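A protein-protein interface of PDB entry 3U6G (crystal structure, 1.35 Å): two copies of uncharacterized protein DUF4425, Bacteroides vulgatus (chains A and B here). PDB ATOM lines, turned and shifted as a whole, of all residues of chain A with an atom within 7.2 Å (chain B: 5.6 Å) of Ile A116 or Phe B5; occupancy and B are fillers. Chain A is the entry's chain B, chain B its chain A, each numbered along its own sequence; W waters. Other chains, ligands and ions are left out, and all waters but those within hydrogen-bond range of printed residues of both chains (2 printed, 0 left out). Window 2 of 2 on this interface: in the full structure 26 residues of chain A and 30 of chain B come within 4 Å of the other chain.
Of the 11 printed residues of chain A, 4 touch a printed residue of chain B.
Printed residues of chain A that touch a printed residue of chain B: Ser A77, Thr A114, Ile A116 and Thr A118.
Hydrophobic or aromatic side chains of chain A that line the printed part of chain B: Ile A116.
Of the 11 printed residues of chain B, 5 touch a printed residue of chain A.
Among the printed residues, 8 pairs touch across the chains.
Among the printed residues, no Asp or Glu carboxylate lies within 4 Å of a Lys or Arg side-chain nitrogen of the other chain.
Ile A116 touches just these residues of chain B: Ala B2 (3.8 Å), Phe B5 (3.4 Å) and Phe B70 (3.5 Å).
Phe B5 touches just these residues of chain A: Ile A116 and Thr A118.
Printed residues of chain A within 4 Å of Ala B2: Thr A114 and Ile A116.
Of the printed residues of chain B, Thr A118 touches Phe B5, Phe B71 and Lys B124.
Of the printed residues of chain A, Lys B124 touches Thr A118 (3.8 Å).
Val A78 touches none of the printed residues of chain B.
Ser B3 touches none of the printed residues of chain A.
The nearest residue of chain A that does not touch Phe B5 is Glu A117 (4.4 Å).
The nearest printed residue of chain A that does not touch Phe B70 is Ser A79 (4.3 Å).
No position is printed for both chains.
Among the printed residues, merely in contact across the chains: Ser A77 with Phe B70 (3.3 Å), Ile A116 with Phe B5 (3.4 Å), Ile A116 with Phe B70 (3.5 Å), Thr A114 with Ala B2 (3.6 Å), Thr A118 with Phe B5 (3.6 Å), Thr A118 with Phe B71 (3.7 Å), Thr A118 with Lys B124 (3.8 Å) and Ile A116 with Ala B2 (3.8 Å).
Water W2 lies within hydrogen-bond range of NZ of Lys B124 (2.7 Å), OE1 of Glu A117 (2.8 Å) and N of Thr A118 (2.9 Å).
Water W1 lies within hydrogen-bond range of OG of Ser A79 and O of Lys B34.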
ATOM      1  N   SER A  77      27.366 -20.874  12.210  1.00  0.00           N
ATOM      2  CA  SER A  77      27.002 -20.821  10.799  1.00  0.00           C
ATOM      3  C   SER A  77      28.271 -20.877   9.973  1.00  0.00           C
ATOM      4  O   SER A  77      29.238 -20.196  10.300  1.00  0.00           O
ATOM      5  CB  SER A  77      26.263 -19.516  10.494  1.00  0.00           C
ATOM      6  OG  SER A  77      25.953 -19.410   9.116  1.00  0.00           O
ATOM      7  N   VAL A  78      28.249 -21.665   8.907  1.00  0.00           N
ATOM      8  CA  VAL A  78      29.370 -21.777   7.980  1.00  0.00           C
ATOM      9  C   VAL A  78      28.805 -21.536   6.605  1.00  0.00           C
ATOM     10  O   VAL A  78      27.843 -22.189   6.197  1.00  0.00           O
ATOM     11  CB  VAL A  78      29.997 -23.172   8.051  1.00  0.00           C
ATOM     12  CG1 VAL A  78      31.086 -23.363   6.977  1.00  0.00           C
ATOM     13  CG2 VAL A  78      30.529 -23.440   9.457  1.00  0.00           C
ATOM     14  N   SER A  79      29.391 -20.591   5.881  1.00  0.00           N
ATOM     15  CA  SER A  79      28.924 -20.313   4.530  1.00  0.00           C
ATOM     16  C   SER A  79      30.081 -20.081   3.578  1.00  0.00           C
ATOM     17  O   SER A  79      31.158 -19.678   3.995  1.00  0.00           O
ATOM     18  CB  SER A  79      27.916 -19.146   4.502  1.00  0.00           C
ATOM     19  OG  SER A  79      28.483 -17.950   4.981  1.00  0.00           O
ATOM     20  N   SER A  80      29.847 -20.351   2.301  1.00  0.00           N
ATOM     21  CA  SER A  80      30.848 -20.108   1.273  1.00  0.00           C
ATOM     22  C   SER A  80      30.167 -19.916  -0.075  1.00  0.00           C
ATOM     23  O   SER A  80      29.175 -20.587  -0.371  1.00  0.00           O
ATOM     24  CB  SER A  80      31.836 -21.277   1.179  1.00  0.00           C
ATOM     25  OG  SER A  80      32.814 -21.028   0.190  1.00  0.00           O
ATOM     26  N   TYR A 108      33.409 -29.731   5.899  1.00  0.00           N
ATOM     27  CA  TYR A 108      32.630 -29.083   4.866  1.00  0.00           C
ATOM     28  C   TYR A 108      33.480 -29.009   3.620  1.00  0.00           C
ATOM     29  O   TYR A 108      34.666 -28.692   3.676  1.00  0.00           O
ATOM     30  CB  TYR A 108      32.222 -27.672   5.305  1.00  0.00           C
ATOM     31  CG  TYR A 108      31.451 -27.654   6.615  1.00  0.00           C
ATOM     32  CD1 TYR A 108      30.111 -28.030   6.663  1.00  0.00           C
ATOM     33  CD2 TYR A 108      32.054 -27.259   7.798  1.00  0.00           C
ATOM     34  CE1 TYR A 108      29.401 -28.016   7.848  1.00  0.00           C
ATOM     35  CE2 TYR A 108      31.353 -27.245   8.989  1.00  0.00           C
ATOM     36  CZ  TYR A 108      30.023 -27.617   9.011  1.00  0.00           C
ATOM     37  OH  TYR A 108      29.315 -27.607  10.200  1.00  0.00           O
ATOM     38  N   ASN A 113      28.289 -24.941  -5.712  1.00  0.00           N
ATOM     39  CA  ASN A 113      27.080 -24.257  -5.256  1.00  0.00           C
ATOM     40  C   ASN A 113      27.336 -23.498  -3.976  1.00  0.00           C
ATOM     41  O   ASN A 113      28.321 -23.743  -3.284  1.00  0.00           O
ATOM     42  CB  ASN A 113      25.967 -25.267  -4.959  1.00  0.00           C
ATOM     43  CG  ASN A 113      25.582 -26.098  -6.167  1.00  0.00           C
ATOM     44  OD1 ASN A 113      25.490 -27.326  -6.081  1.00  0.00           O
ATOM     45  ND2 ASN A 113      25.351 -25.439  -7.297  1.00  0.00           N
ATOM     46  N   THR A 114      26.421 -22.605  -3.629  1.00  0.00           N
ATOM     47  CA  THR A 114      26.485 -21.916  -2.348  1.00  0.00           C
ATOM     48  C   THR A 114      26.400 -22.950  -1.237  1.00  0.00           C
ATOM     49  O   THR A 114      25.549 -23.850  -1.286  1.00  0.00           O
ATOM     50  CB  THR A 114      25.327 -20.919  -2.191  1.00  0.00           C
ATOM     51  OG1 THR A 114      25.239 -20.107  -3.369  1.00  0.00           O
ATOM     52  CG2 THR A 114      25.535 -20.031  -0.952  1.00  0.00           C
ATOM     53  N   LEU A 115      27.290 -22.831  -0.253  1.00  0.00           N
ATOM     54  CA  LEU A 115      27.294 -23.700   0.911  1.00  0.00           C
ATOM     55  C   LEU A 115      26.787 -22.886   2.091  1.00  0.00           C
ATOM     56  O   LEU A 115      27.272 -21.791   2.345  1.00  0.00           O
ATOM     57  CB  LEU A 115      28.714 -24.241   1.174  1.00  0.00           C
ATOM     58  CG  LEU A 115      28.869 -25.233   2.329  1.00  0.00           C
ATOM     59  CD1 LEU A 115      29.975 -26.249   2.010  1.00  0.00           C
ATOM     60  CD2 LEU A 115      29.171 -24.527   3.653  1.00  0.00           C
ATOM     61  N   ILE A 116      25.776 -23.415   2.771  1.00  0.00           N
ATOM     62  CA  ILE A 116      25.321 -22.863   4.057  1.00  0.00           C
ATOM     63  C   ILE A 116      25.008 -24.039   4.969  1.00  0.00           C
ATOM     64  O   ILE A 116      24.195 -24.903   4.622  1.00  0.00           O
ATOM     65  CB  ILE A 116      24.054 -22.000   3.964  1.00  0.00           C
ATOM     66  CG1 ILE A 116      24.183 -20.927   2.880  1.00  0.00           C
ATOM     67  CG2 ILE A 116      23.762 -21.345   5.330  1.00  0.00           C
ATOM     68  CD1 ILE A 116      22.893 -20.121   2.635  1.00  0.00           C
ATOM     69  N   GLU A 117      25.665 -24.077   6.126  1.00  0.00           N
ATOM     70  CA  GLU A 117      25.426 -25.132   7.110  1.00  0.00           C
ATOM     71  C   GLU A 117      25.460 -24.504   8.479  1.00  0.00           C
ATOM     72  O   GLU A 117      26.098 -23.475   8.664  1.00  0.00           O
ATOM     73  CB  GLU A 117      26.509 -26.210   7.016  1.00  0.00           C
ATOM     74  CG  GLU A 117      26.669 -26.862   5.632  1.00  0.00           C
ATOM     75  CD  GLU A 117      25.510 -27.768   5.237  1.00  0.00           C
ATOM     76  OE1 GLU A 117      24.784 -28.249   6.134  1.00  0.00           O
ATOM     77  OE2 GLU A 117      25.331 -28.017   4.017  1.00  0.00           O
ATOM     78  N   THR A 118      24.799 -25.139   9.441  1.00  0.00           N
ATOM     79  CA  THR A 118      24.816 -24.660  10.808  1.00  0.00           C
ATOM     80  C   THR A 118      25.134 -25.804  11.763  1.00  0.00           C
ATOM     81  O   THR A 118      25.018 -26.984  11.427  1.00  0.00           O
ATOM     82  CB  THR A 118      23.471 -24.016  11.192  1.00  0.00           C
ATOM     83  OG1 THR A 118      22.420 -24.973  11.012  1.00  0.00           O
ATOM     84  CG2 THR A 118      23.213 -22.759  10.335  1.00  0.00           C
ATOM     85  N   ALA B   2      21.757 -25.372   1.687  1.00  0.00           N
ATOM     86  CA  ALA B   2      21.499 -23.924   1.430  1.00  0.00           C
ATOM     87  C   ALA B   2      20.023 -23.648   1.156  1.00  0.00           C
ATOM     88  O   ALA B   2      19.529 -22.558   1.455  1.00  0.00           O
ATOM     89  CB  ALA B   2      22.366 -23.416   0.275  1.00  0.00           C
ATOM     90  N   SER B   3      19.320 -24.639   0.610  1.00  0.00           N
ATOM     91  CA  SER B   3      17.889 -24.511   0.318  1.00  0.00           C
ATOM     92  C   SER B   3      17.046 -24.421   1.592  1.00  0.00           C
ATOM     93  O   SER B   3      15.905 -23.967   1.543  1.00  0.00           O
ATOM     94  CB  SER B   3      17.402 -25.676  -0.564  1.00  0.00           C
ATOM     95  OG  SER B   3      17.554 -26.931   0.085  1.00  0.00           O
ATOM     96  N   ASP B   4      17.613 -24.836   2.728  1.00  0.00           N
ATOM     97  CA  ASP B   4      16.924 -24.780   4.025  1.00  0.00           C
ATOM     98  C   ASP B   4      16.952 -23.389   4.657  1.00  0.00           C
ATOM     99  O   ASP B   4      16.358 -23.176   5.735  1.00  0.00           O
ATOM    100  CB  ASP B   4      17.558 -25.767   5.013  1.00  0.00           C
ATOM    101  CG  ASP B   4      17.471 -27.204   4.543  1.00  0.00           C
ATOM    102  OD1 ASP B   4      16.525 -27.522   3.788  1.00  0.00           O
ATOM    103  OD2 ASP B   4      18.345 -28.013   4.939  1.00  0.00           O
ATOM    104  N   PHE B   5      17.651 -22.457   4.006  1.00  0.00           N
ATOM    105  CA  PHE B   5      17.795 -21.104   4.508  1.00  0.00           C
ATOM    106  C   PHE B   5      17.159 -20.108   3.538  1.00  0.00           C
ATOM    107  O   PHE B   5      17.188 -20.290   2.313  1.00  0.00           O
ATOM    108  CB  PHE B   5      19.275 -20.781   4.730  1.00  0.00           C
ATOM    109  CG  PHE B   5      19.974 -21.754   5.627  1.00  0.00           C
ATOM    110  CD1 PHE B   5      20.595 -22.879   5.104  1.00  0.00           C
ATOM    111  CD2 PHE B   5      20.009 -21.559   6.992  1.00  0.00           C
ATOM    112  CE1 PHE B   5      21.242 -23.781   5.931  1.00  0.00           C
ATOM    113  CE2 PHE B   5      20.636 -22.450   7.825  1.00  0.00           C
ATOM    114  CZ  PHE B   5      21.266 -23.572   7.290  1.00  0.00           C
ATOM    115  N   GLN B   6      16.550 -19.078   4.102  1.00  0.00           N
ATOM    116  CA  GLN B   6      15.944 -18.015   3.336  1.00  0.00           C
ATOM    117  C   GLN B   6      16.452 -16.695   3.894  1.00  0.00           C
ATOM    118  O   GLN B   6      16.523 -16.524   5.105  1.00  0.00           O
ATOM    119  CB  GLN B   6      14.430 -18.101   3.485  1.00  0.00           C
ATOM    120  CG  GLN B   6      13.642 -17.076   2.691  1.00  0.00           C
ATOM    121  CD  GLN B   6      12.142 -17.369   2.681  1.00  0.00           C
ATOM    122  OE1 GLN B   6      11.682 -18.417   3.161  1.00  0.00           O
ATOM    123  NE2 GLN B   6      11.376 -16.444   2.130  1.00  0.00           N
ATOM    124  N   THR B   7      16.810 -15.783   3.007  1.00  0.00           N
ATOM    125  CA  THR B   7      17.235 -14.462   3.404  1.00  0.00           C
ATOM    126  C   THR B   7      15.986 -13.604   3.611  1.00  0.00           C
ATOM    127  O   THR B   7      15.020 -13.705   2.852  1.00  0.00           O
ATOM    128  CB  THR B   7      18.186 -13.883   2.360  1.00  0.00           C
ATOM    129  OG1 THR B   7      19.356 -14.720   2.282  1.00  0.00           O
ATOM    130  CG2 THR B   7      18.584 -12.468   2.724  1.00  0.00           C
ATOM    131  N   LYS B  34      25.675 -13.105   5.385  1.00  0.00           N
ATOM    132  CA  LYS B  34      26.810 -13.569   4.593  1.00  0.00           C
ATOM    133  C   LYS B  34      28.151 -12.952   5.029  1.00  0.00           C
ATOM    134  O   LYS B  34      29.211 -13.455   4.651  1.00  0.00           O
ATOM    135  CB  LYS B  34      26.566 -13.331   3.094  1.00  0.00           C
ATOM    136  CG  LYS B  34      25.586 -14.309   2.431  1.00  0.00           C
ATOM    137  CD  LYS B  34      26.220 -15.684   2.181  1.00  0.00           C
ATOM    138  CE  LYS B  34      25.443 -16.518   1.178  1.00  0.00           C
ATOM    139  NZ  LYS B  34      23.972 -16.456   1.367  1.00  0.00           N
ATOM    140  N   PHE B  70      20.155 -14.934   7.106  1.00  0.00           N
ATOM    141  CA  PHE B  70      19.661 -16.192   6.537  1.00  0.00           C
ATOM    142  C   PHE B  70      19.403 -17.244   7.599  1.00  0.00           C
ATOM    143  O   PHE B  70      18.955 -18.330   7.276  1.00  0.00           O
ATOM    144  CB  PHE B  70      20.567 -16.730   5.423  1.00  0.00           C
ATOM    145  CG  PHE B  70      21.981 -16.994   5.850  1.00  0.00           C
ATOM    146  CD1 PHE B  70      22.269 -18.071   6.674  1.00  0.00           C
ATOM    147  CD2 PHE B  70      23.022 -16.172   5.447  1.00  0.00           C
ATOM    148  CE1 PHE B  70      23.568 -18.342   7.072  1.00  0.00           C
ATOM    149  CE2 PHE B  70      24.323 -16.451   5.840  1.00  0.00           C
ATOM    150  CZ  PHE B  70      24.586 -17.511   6.679  1.00  0.00           C
ATOM    151  N   PHE B  71      19.626 -16.902   8.868  1.00  0.00           N
ATOM    152  CA  PHE B  71      19.514 -17.821   9.976  1.00  0.00           C
ATOM    153  C   PHE B  71      19.428 -17.049  11.279  1.00  0.00           C
ATOM    154  O   PHE B  71      20.096 -16.034  11.440  1.00  0.00           O
ATOM    155  CB  PHE B  71      20.755 -18.700  10.008  1.00  0.00           C
ATOM    156  CG  PHE B  71      20.764 -19.747  11.091  1.00  0.00           C
ATOM    157  CD1 PHE B  71      19.838 -20.779  11.098  1.00  0.00           C
ATOM    158  CD2 PHE B  71      21.745 -19.730  12.069  1.00  0.00           C
ATOM    159  CE1 PHE B  71      19.856 -21.763  12.086  1.00  0.00           C
ATOM    160  CE2 PHE B  71      21.783 -20.720  13.067  1.00  0.00           C
ATOM    161  CZ  PHE B  71      20.836 -21.745  13.063  1.00  0.00           C
ATOM    162  N   LYS B 124      15.890 -22.177  10.553  1.00  0.00           N
ATOM    163  CA  LYS B 124      16.236 -23.127   9.486  1.00  0.00           C
ATOM    164  C   LYS B 124      15.094 -24.119   9.277  1.00  0.00           C
ATOM    165  O   LYS B 124      14.515 -24.618  10.247  1.00  0.00           O
ATOM    166  CB  LYS B 124      17.517 -23.890   9.853  1.00  0.00           C
ATOM    167  CG  LYS B 124      17.940 -24.966   8.863  1.00  0.00           C
ATOM    168  CD  LYS B 124      19.126 -25.770   9.378  1.00  0.00           C
ATOM    169  CE  LYS B 124      19.368 -27.004   8.523  1.00  0.00           C
ATOM    170  NZ  LYS B 124      20.679 -27.642   8.835  1.00  0.00           N
ATOM    171  N   GLU B 125      14.806 -24.436   8.016  1.00  0.00           N
ATOM    172  CA  GLU B 125      13.776 -25.427   7.671  1.00  0.00           C
ATOM    173  C   GLU B 125      14.172 -26.803   8.211  1.00  0.00           C
ATOM    174  O   GLU B 125      15.241 -27.320   7.869  1.00  0.00           O
ATOM    175  CB  GLU B 125      13.558 -25.493   6.151  1.00  0.00           C
HETATM  176  O   HOH W   1      29.232 -15.972   3.305  1.00  0.00           O
HETATM  177  O   HOH W   2      23.342 -27.477   8.436  1.00  0.00           O
